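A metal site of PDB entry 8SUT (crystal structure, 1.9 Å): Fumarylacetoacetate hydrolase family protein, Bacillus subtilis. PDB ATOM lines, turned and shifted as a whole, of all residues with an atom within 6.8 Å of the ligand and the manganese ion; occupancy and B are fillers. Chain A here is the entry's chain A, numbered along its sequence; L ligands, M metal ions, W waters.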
ATOM      1  N   CYS A  99      13.574 -17.447 -17.190  1.00  0.00           N
ATOM      2  CA  CYS A  99      14.837 -18.142 -17.360  1.00  0.00           C
ATOM      3  C   CYS A  99      14.621 -19.595 -17.740  1.00  0.00           C
ATOM      4  O   CYS A  99      13.757 -20.276 -17.188  1.00  0.00           O
ATOM      5  CB  CYS A  99      15.674 -18.060 -16.096  1.00  0.00           C
ATOM      6  SG  CYS A  99      16.069 -16.395 -15.576  1.00  0.00           S
ATOM      7  N   ILE A 100      15.420 -20.049 -18.718  1.00  0.00           N
ATOM      8  CA  ILE A 100      15.439 -21.441 -19.125  1.00  0.00           C
ATOM      9  C   ILE A 100      16.619 -22.121 -18.434  1.00  0.00           C
ATOM     10  O   ILE A 100      17.736 -21.608 -18.446  1.00  0.00           O
ATOM     11  CB  ILE A 100      15.490 -21.586 -20.661  1.00  0.00           C
ATOM     12  CG1 ILE A 100      14.510 -20.620 -21.351  1.00  0.00           C
ATOM     13  CG2 ILE A 100      15.250 -23.042 -21.095  1.00  0.00           C
ATOM     14  CD1 ILE A 100      12.989 -20.786 -20.928  1.00  0.00           C
ATOM     15  N   GLY A 101      16.345 -23.271 -17.811  1.00  0.00           N
ATOM     16  CA  GLY A 101      17.385 -24.121 -17.264  1.00  0.00           C
ATOM     17  C   GLY A 101      17.819 -25.225 -18.226  1.00  0.00           C
ATOM     18  O   GLY A 101      16.974 -25.786 -18.927  1.00  0.00           O
ATOM     19  N   LYS A 102      19.115 -25.534 -18.233  1.00  0.00           N
ATOM     20  CA  LYS A 102      19.645 -26.678 -18.966  1.00  0.00           C
ATOM     21  C   LYS A 102      19.169 -26.707 -20.413  1.00  0.00           C
ATOM     22  O   LYS A 102      18.467 -27.624 -20.835  1.00  0.00           O
ATOM     23  CB  LYS A 102      19.247 -27.988 -18.266  1.00  0.00           C
ATOM     24  CG  LYS A 102      19.720 -28.084 -16.806  1.00  0.00           C
ATOM     25  CD  LYS A 102      19.318 -29.399 -16.129  1.00  0.00           C
ATOM     26  CE  LYS A 102      20.357 -29.924 -15.160  1.00  0.00           C
ATOM     27  NZ  LYS A 102      20.780 -28.892 -14.165  1.00  0.00           N
ATOM     28  N   ASN A 103      19.575 -25.691 -21.185  1.00  0.00           N
ATOM     29  CA  ASN A 103      19.219 -25.608 -22.592  1.00  0.00           C
ATOM     30  C   ASN A 103      20.421 -25.841 -23.498  1.00  0.00           C
ATOM     31  O   ASN A 103      20.329 -25.674 -24.714  1.00  0.00           O
ATOM     32  CB  ASN A 103      18.559 -24.251 -22.870  1.00  0.00           C
ATOM     33  CG  ASN A 103      17.740 -24.232 -24.154  1.00  0.00           C
ATOM     34  OD1 ASN A 103      17.180 -25.247 -24.535  1.00  0.00           O
ATOM     35  ND2 ASN A 103      17.652 -23.088 -24.828  1.00  0.00           N
ATOM     36  N   TYR A 104      21.568 -26.196 -22.891  1.00  0.00           N
ATOM     37  CA  TYR A 104      22.745 -26.651 -23.626  1.00  0.00           C
ATOM     38  C   TYR A 104      23.120 -28.025 -23.059  1.00  0.00           C
ATOM     39  O   TYR A 104      23.189 -28.186 -21.844  1.00  0.00           O
ATOM     40  CB  TYR A 104      23.943 -25.713 -23.487  1.00  0.00           C
ATOM     41  CG  TYR A 104      23.812 -24.399 -24.219  1.00  0.00           C
ATOM     42  CD1 TYR A 104      22.993 -23.386 -23.723  1.00  0.00           C
ATOM     43  CD2 TYR A 104      24.544 -24.145 -25.367  1.00  0.00           C
ATOM     44  CE1 TYR A 104      22.873 -22.163 -24.375  1.00  0.00           C
ATOM     45  CE2 TYR A 104      24.452 -22.915 -26.016  1.00  0.00           C
ATOM     46  CZ  TYR A 104      23.609 -21.926 -25.512  1.00  0.00           C
ATOM     47  OH  TYR A 104      23.469 -20.695 -26.124  1.00  0.00           O
ATOM     48  N   HIS A 107      26.001 -28.265 -20.482  1.00  0.00           N
ATOM     49  CA  HIS A 107      25.676 -27.645 -19.201  1.00  0.00           C
ATOM     50  C   HIS A 107      24.899 -28.630 -18.321  1.00  0.00           C
ATOM     51  O   HIS A 107      25.199 -28.765 -17.130  1.00  0.00           O
ATOM     52  CB  HIS A 107      24.843 -26.367 -19.350  1.00  0.00           C
ATOM     53  CG  HIS A 107      24.533 -25.763 -18.023  1.00  0.00           C
ATOM     54  ND1 HIS A 107      25.546 -25.368 -17.186  1.00  0.00           N
ATOM     55  CD2 HIS A 107      23.380 -25.556 -17.348  1.00  0.00           C
ATOM     56  CE1 HIS A 107      25.015 -24.917 -16.042  1.00  0.00           C
ATOM     57  NE2 HIS A 107      23.706 -25.005 -16.127  1.00  0.00           N
ATOM     58  N   ALA A 108      23.879 -29.282 -18.913  1.00  0.00           N
ATOM     59  CA  ALA A 108      23.085 -30.299 -18.251  1.00  0.00           C
ATOM     60  C   ALA A 108      23.945 -31.447 -17.711  1.00  0.00           C
ATOM     61  O   ALA A 108      23.726 -31.922 -16.586  1.00  0.00           O
ATOM     62  CB  ALA A 108      22.025 -30.831 -19.213  1.00  0.00           C
ATOM     63  N   MET A 111      26.246 -30.567 -14.690  1.00  0.00           N
ATOM     64  CA  MET A 111      25.467 -30.363 -13.465  1.00  0.00           C
ATOM     65  C   MET A 111      24.893 -31.680 -12.921  1.00  0.00           C
ATOM     66  O   MET A 111      24.172 -31.665 -11.924  1.00  0.00           O
ATOM     67  CB  MET A 111      24.306 -29.350 -13.727  1.00  0.00           C
ATOM     68  CG  MET A 111      24.781 -27.927 -14.065  1.00  0.00           C
ATOM     69  SD  MET A 111      25.719 -27.062 -12.758  1.00  0.00           S
ATOM     70  CE  MET A 111      24.482 -27.019 -11.411  1.00  0.00           C
ATOM     71  N   MET A 122      12.708 -26.378 -18.872  1.00  0.00           N
ATOM     72  CA  MET A 122      12.568 -26.119 -17.448  1.00  0.00           C
ATOM     73  C   MET A 122      12.601 -24.594 -17.328  1.00  0.00           C
ATOM     74  O   MET A 122      13.594 -23.977 -17.704  1.00  0.00           O
ATOM     75  CB  MET A 122      13.676 -26.853 -16.684  1.00  0.00           C
ATOM     76  CG  MET A 122      14.156 -26.184 -15.426  1.00  0.00           C
ATOM     77  SD  MET A 122      15.470 -27.145 -14.599  1.00  0.00           S
ATOM     78  CE  MET A 122      14.681 -28.686 -14.354  1.00  0.00           C
ATOM     79  N   PHE A 124      11.961 -21.093 -14.996  1.00  0.00           N
ATOM     80  CA  PHE A 124      11.829 -20.426 -13.710  1.00  0.00           C
ATOM     81  C   PHE A 124      12.037 -18.927 -13.925  1.00  0.00           C
ATOM     82  O   PHE A 124      12.188 -18.470 -15.055  1.00  0.00           O
ATOM     83  CB  PHE A 124      12.821 -21.053 -12.712  1.00  0.00           C
ATOM     84  CG  PHE A 124      14.227 -20.882 -13.183  1.00  0.00           C
ATOM     85  CD1 PHE A 124      14.799 -21.794 -14.062  1.00  0.00           C
ATOM     86  CD2 PHE A 124      14.969 -19.780 -12.807  1.00  0.00           C
ATOM     87  CE1 PHE A 124      16.094 -21.627 -14.516  1.00  0.00           C
ATOM     88  CE2 PHE A 124      16.265 -19.611 -13.278  1.00  0.00           C
ATOM     89  CZ  PHE A 124      16.817 -20.535 -14.131  1.00  0.00           C
ATOM     90  N   GLU A 151      26.591 -17.223 -14.905  1.00  0.00           N
ATOM     91  CA  GLU A 151      26.008 -17.867 -16.085  1.00  0.00           C
ATOM     92  C   GLU A 151      25.803 -16.853 -17.213  1.00  0.00           C
ATOM     93  O   GLU A 151      24.866 -16.052 -17.166  1.00  0.00           O
ATOM     94  CB  GLU A 151      24.651 -18.493 -15.726  1.00  0.00           C
ATOM     95  CG  GLU A 151      24.665 -19.550 -14.637  1.00  0.00           C
ATOM     96  CD  GLU A 151      23.349 -20.291 -14.476  1.00  0.00           C
ATOM     97  OE1 GLU A 151      22.414 -19.918 -15.208  1.00  0.00           O
ATOM     98  OE2 GLU A 151      23.255 -21.241 -13.675  1.00  0.00           O
ATOM     99  N   GLY A 152      26.662 -16.857 -18.224  1.00  0.00           N
ATOM    100  CA  GLY A 152      26.464 -15.998 -19.370  1.00  0.00           C
ATOM    101  C   GLY A 152      25.347 -16.530 -20.254  1.00  0.00           C
ATOM    102  O   GLY A 152      25.332 -17.727 -20.548  1.00  0.00           O
ATOM    103  N   GLU A 153      24.408 -15.670 -20.649  1.00  0.00           N
ATOM    104  CA  GLU A 153      23.290 -16.082 -21.493  1.00  0.00           C
ATOM    105  C   GLU A 153      22.864 -15.024 -22.508  1.00  0.00           C
ATOM    106  O   GLU A 153      23.029 -13.813 -22.285  1.00  0.00           O
ATOM    107  CB  GLU A 153      22.042 -16.423 -20.662  1.00  0.00           C
ATOM    108  CG  GLU A 153      22.380 -17.181 -19.424  1.00  0.00           C
ATOM    109  CD  GLU A 153      21.207 -17.829 -18.724  1.00  0.00           C
ATOM    110  OE1 GLU A 153      20.063 -17.848 -19.258  1.00  0.00           O
ATOM    111  OE2 GLU A 153      21.450 -18.315 -17.614  1.00  0.00           O
ATOM    112  N   ASP A 182      23.151 -14.643 -15.383  1.00  0.00           N
ATOM    113  CA  ASP A 182      22.178 -15.231 -14.470  1.00  0.00           C
ATOM    114  C   ASP A 182      22.892 -15.754 -13.224  1.00  0.00           C
ATOM    115  O   ASP A 182      23.029 -16.958 -13.028  1.00  0.00           O
ATOM    116  CB  ASP A 182      21.404 -16.348 -15.203  1.00  0.00           C
ATOM    117  CG  ASP A 182      20.392 -17.117 -14.353  1.00  0.00           C
ATOM    118  OD1 ASP A 182      20.035 -16.648 -13.243  1.00  0.00           O
ATOM    119  OD2 ASP A 182      19.967 -18.175 -14.793  1.00  0.00           O
ATOM    120  N   THR A 184      23.703 -16.992  -9.682  1.00  0.00           N
ATOM    121  CA  THR A 184      22.952 -17.978  -8.928  1.00  0.00           C
ATOM    122  C   THR A 184      23.670 -18.375  -7.636  1.00  0.00           C
ATOM    123  O   THR A 184      24.884 -18.577  -7.633  1.00  0.00           O
ATOM    124  CB  THR A 184      22.748 -19.214  -9.829  1.00  0.00           C
ATOM    125  OG1 THR A 184      22.151 -18.794 -11.071  1.00  0.00           O
ATOM    126  CG2 THR A 184      21.886 -20.301  -9.177  1.00  0.00           C
ATOM    127  N   ARG A 186      24.047 -21.428  -5.587  1.00  0.00           N
ATOM    128  CA  ARG A 186      23.796 -22.838  -5.867  1.00  0.00           C
ATOM    129  C   ARG A 186      23.268 -23.625  -4.665  1.00  0.00           C
ATOM    130  O   ARG A 186      22.478 -24.568  -4.827  1.00  0.00           O
ATOM    131  CB  ARG A 186      25.091 -23.535  -6.319  1.00  0.00           C
ATOM    132  CG  ARG A 186      25.672 -22.985  -7.631  1.00  0.00           C
ATOM    133  CD  ARG A 186      24.917 -23.513  -8.812  1.00  0.00           C
ATOM    134  NE  ARG A 186      25.428 -22.946 -10.051  1.00  0.00           N
ATOM    135  CZ  ARG A 186      24.698 -22.748 -11.157  1.00  0.00           C
ATOM    136  NH1 ARG A 186      23.431 -23.119 -11.229  1.00  0.00           N
ATOM    137  NH2 ARG A 186      25.283 -22.181 -12.212  1.00  0.00           N
ATOM    138  N   GLN A 189      19.579 -22.734  -4.332  1.00  0.00           N
ATOM    139  CA  GLN A 189      18.844 -23.530  -5.297  1.00  0.00           C
ATOM    140  C   GLN A 189      18.455 -24.899  -4.769  1.00  0.00           C
ATOM    141  O   GLN A 189      17.312 -25.342  -4.945  1.00  0.00           O
ATOM    142  CB  GLN A 189      19.660 -23.776  -6.564  1.00  0.00           C
ATOM    143  CG  GLN A 189      19.591 -22.745  -7.618  1.00  0.00           C
ATOM    144  CD  GLN A 189      20.273 -23.283  -8.860  1.00  0.00           C
ATOM    145  OE1 GLN A 189      21.479 -23.562  -8.864  1.00  0.00           O
ATOM    146  NE2 GLN A 189      19.533 -23.451  -9.934  1.00  0.00           N
ATOM    147  N   PHE A 195      13.863 -22.835  -7.897  1.00  0.00           N
ATOM    148  CA  PHE A 195      15.048 -22.016  -8.076  1.00  0.00           C
ATOM    149  C   PHE A 195      14.907 -20.543  -7.727  1.00  0.00           C
ATOM    150  O   PHE A 195      15.907 -19.830  -7.624  1.00  0.00           O
ATOM    151  CB  PHE A 195      15.488 -22.126  -9.545  1.00  0.00           C
ATOM    152  CG  PHE A 195      16.066 -23.449  -9.989  1.00  0.00           C
ATOM    153  CD1 PHE A 195      16.312 -24.468  -9.057  1.00  0.00           C
ATOM    154  CD2 PHE A 195      16.347 -23.687 -11.316  1.00  0.00           C
ATOM    155  CE1 PHE A 195      16.857 -25.684  -9.470  1.00  0.00           C
ATOM    156  CE2 PHE A 195      16.881 -24.915 -11.725  1.00  0.00           C
ATOM    157  CZ  PHE A 195      17.131 -25.898 -10.796  1.00  0.00           C
ATOM    158  N   LYS A 199      17.963 -17.735  -7.353  1.00  0.00           N
ATOM    159  CA  LYS A 199      18.071 -16.925  -8.554  1.00  0.00           C
ATOM    160  C   LYS A 199      17.736 -15.447  -8.356  1.00  0.00           C
ATOM    161  O   LYS A 199      18.007 -14.628  -9.239  1.00  0.00           O
ATOM    162  CB  LYS A 199      17.128 -17.497  -9.623  1.00  0.00           C
ATOM    163  CG  LYS A 199      17.518 -18.871 -10.117  1.00  0.00           C
ATOM    164  CD  LYS A 199      18.695 -18.803 -11.034  1.00  0.00           C
ATOM    165  CE  LYS A 199      19.088 -20.154 -11.549  1.00  0.00           C
ATOM    166  NZ  LYS A 199      20.127 -20.033 -12.579  1.00  0.00           N
ATOM    167  N   ALA A 266      15.792 -15.238 -20.747  1.00  0.00           N
ATOM    168  CA  ALA A 266      17.162 -15.726 -20.684  1.00  0.00           C
ATOM    169  C   ALA A 266      17.169 -17.192 -21.128  1.00  0.00           C
ATOM    170  O   ALA A 266      16.568 -18.031 -20.463  1.00  0.00           O
ATOM    171  CB  ALA A 266      17.694 -15.577 -19.258  1.00  0.00           C
ATOM    172  N   THR A 267      17.887 -17.483 -22.218  1.00  0.00           N
ATOM    173  CA  THR A 267      17.738 -18.736 -22.938  1.00  0.00           C
ATOM    174  C   THR A 267      18.654 -19.875 -22.481  1.00  0.00           C
ATOM    175  O   THR A 267      18.713 -20.916 -23.129  1.00  0.00           O
ATOM    176  CB  THR A 267      17.920 -18.432 -24.457  1.00  0.00           C
ATOM    177  OG1 THR A 267      19.226 -17.902 -24.682  1.00  0.00           O
ATOM    178  CG2 THR A 267      16.900 -17.460 -24.951  1.00  0.00           C
ATOM    179  N   GLY A 268      19.375 -19.676 -21.370  1.00  0.00           N
ATOM    180  CA  GLY A 268      20.183 -20.735 -20.785  1.00  0.00           C
ATOM    181  C   GLY A 268      21.665 -20.522 -21.062  1.00  0.00           C
ATOM    182  O   GLY A 268      22.046 -19.932 -22.063  1.00  0.00           O
ATOM    183  N   THR A 269      22.485 -21.019 -20.121  1.00  0.00           N
ATOM    184  CA  THR A 269      23.932 -20.835 -20.165  1.00  0.00           C
ATOM    185  C   THR A 269      24.602 -22.082 -20.730  1.00  0.00           C
ATOM    186  O   THR A 269      24.140 -23.204 -20.510  1.00  0.00           O
ATOM    187  CB  THR A 269      24.401 -20.487 -18.743  1.00  0.00           C
ATOM    188  OG1 THR A 269      25.697 -19.911 -18.814  1.00  0.00           O
ATOM    189  CG2 THR A 269      24.419 -21.700 -17.789  1.00  0.00           C
ATOM    190  N   PRO A 270      25.718 -21.949 -21.482  1.00  0.00           N
ATOM    191  CA  PRO A 270      26.520 -23.115 -21.870  1.00  0.00           C
ATOM    192  C   PRO A 270      27.232 -23.750 -20.669  1.00  0.00           C
ATOM    193  O   PRO A 270      27.133 -23.259 -19.542  1.00  0.00           O
ATOM    194  CB  PRO A 270      27.547 -22.540 -22.863  1.00  0.00           C
ATOM    195  CG  PRO A 270      27.139 -21.146 -23.117  1.00  0.00           C
ATOM    196  CD  PRO A 270      26.302 -20.686 -21.961  1.00  0.00           C
ATOM    197  N   VAL A 273      30.241 -23.346 -16.056  1.00  0.00           N
ATOM    198  CA  VAL A 273      29.885 -22.655 -14.822  1.00  0.00           C
ATOM    199  C   VAL A 273      30.820 -23.140 -13.711  1.00  0.00           C
ATOM    200  O   VAL A 273      31.418 -24.217 -13.808  1.00  0.00           O
ATOM    201  CB  VAL A 273      28.387 -22.788 -14.429  1.00  0.00           C
ATOM    202  CG1 VAL A 273      27.483 -22.422 -15.607  1.00  0.00           C
ATOM    203  CG2 VAL A 273      28.048 -24.187 -13.872  1.00  0.00           C
HETATM  204  C1  LIG L   1      21.134 -25.396 -13.394  1.00  0.00           C
HETATM  205  C2  LIG L   1      20.713 -22.535 -16.925  1.00  0.00           C
HETATM  206  C3  LIG L   1      21.047 -23.930 -13.843  1.00  0.00           C
HETATM  207  C4  LIG L   1      19.852 -23.710 -14.743  1.00  0.00           C
HETATM  208  C5  LIG L   1      20.041 -22.418 -15.533  1.00  0.00           C
HETATM  209  O1  LIG L   1      21.791 -26.215 -14.098  1.00  0.00           O
HETATM  210  O2  LIG L   1      20.542 -25.777 -12.347  1.00  0.00           O
HETATM  211  O3  LIG L   1      20.920 -23.641 -17.442  1.00  0.00           O
HETATM  212  O4  LIG L   1      21.057 -21.536 -17.603  1.00  0.00           O
HETATM  213  O5  LIG L   1      20.875 -23.067 -12.747  1.00  0.00           O
HETATM  214  O6  LIG L   1      19.664 -21.376 -15.055  1.00  0.00           O
HETATM  215 MN    MN M   1      20.510 -19.732 -16.327  1.00  0.00          MN
HETATM  216  O   HOH W   1      21.677 -24.104 -19.840  1.00  0.00           O
HETATM  217  O   HOH W   2      18.588 -19.056 -17.464  1.00  0.00           O
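Water W2 lies within hydrogen-bond range of OE1 of Glu 153 (2.6 Å) and O of Ile 100 (2.9 Å). Water W1 lies within hydrogen-bond range of an oxygen (O3) of the ligand (2.6 Å), the backbone carbonyl oxygen (O) of Thr 269 (2.7 Å), the backbone NH (N) of Asn 103 (3.0 Å) and the backbone NH (N) of Lys 102 (3.3 Å).
OE2 of Glu 153 binds the manganese ion, 2.1 Å away. OE1 of Glu 151 binds the manganese ion (2.2 Å). The manganese ion is bound by O6 of the ligand (2.2 Å). The side-chain carboxylate (OD2) of Asp 182 binds the manganese ion, 2.3 Å away. O4 of the ligand is bound to the manganese ion, at 2.3 Å. Water W2 is bound to the manganese ion (2.3 Å).
The side-chain carboxylate (OE1) of Glu 153 lies within hydrogen-bond range of the backbone NH (N) of Gly 268, 2.9 Å away. The side-chain amino group (NZ) of Lys 199 is in salt-bridge range of the side-chain carboxylate (OE2) of Glu 151, at 3.5 Å. The side-chain carboxylate of Glu 151 is in salt-bridge range of the guanidinium group of Arg 186. The backbone carbonyl oxygen (O) of Asp 182 is in hydrogen-bond range of the side-chain hydroxyl (OG1) of Thr 184. OG1 of Thr 269 is in hydrogen-bond range of O of Gly 152, 2.8 Å away. The guanidinium group (NH1) of Arg 186 sits at hydrogen-bond distance from the side-chain amide oxygen (OE1) of Gln 189 (3.1 Å). The backbone NH of Ile 100 sits at hydrogen-bond distance from the backbone carbonyl oxygen of Ala 266 (2.9 Å). N of Gly 101 is in hydrogen-bond range of O of Met 122 (2.8 Å).
O of Ile 100 lies close to O4 of the ligand (3.4 Å). Gly 101 touches the ligand (CA to C4, 3.6 Å). CG of Met 111 touches O1 of the ligand, at 3.4 Å. Phe 124 touches the ligand (CZ to O6, 3.1 Å). CZ of Phe 195 touches O2 of the ligand (3.7 Å). Gly 268 touches the ligand. Hydrophobic or aromatic side chains within 4 Å of the ligand: His 107, Met 111, Phe 124 and Phe 195. 15 residues have an atom within 4 Å of the ligand: Ile 100, Gly 101, Lys 102, His 107, Met 111, Phe 124, Glu 151, Glu 153, Asp 182, Arg 186, Gln 189, Phe 195, Lys 199, Gly 268 and Thr 269. The nearest printed residue that does not touch the ligand is Asn 103 (4.5 Å).
Ile 100 touches the manganese ion. Lys 199 touches the manganese ion (NZ to MN, 3.8 Å). Within 4 Å of the manganese ion: Ile 100, Glu 151, Glu 153, Asp 182 and Lys 199. The nearest printed residue that does not touch the manganese ion is Phe 124 (4.4 Å).
The backbone NH (N) of Lys 102 lies within hydrogen-bond range of an oxygen (O3) of the ligand (2.7 Å). O1 of the ligand is in salt-bridge range of NZ of Lys 102, at 2.9 Å. O5 of the ligand lies within hydrogen-bond range of NZ of Lys 199. An oxygen (O4) of the ligand sits close to the backbone NH (N) of Thr 269, 2.9 Å away. NH1 of Arg 186 is in hydrogen-bond range of O5 of the ligand (3.0 Å). A ring nitrogen (NE2) of His 107 sits at hydrogen-bond distance from an oxygen (O1) of the ligand (3.0 Å). NE2 of Gln 189 is in hydrogen-bond range of O5 of the ligand (3.1 Å).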
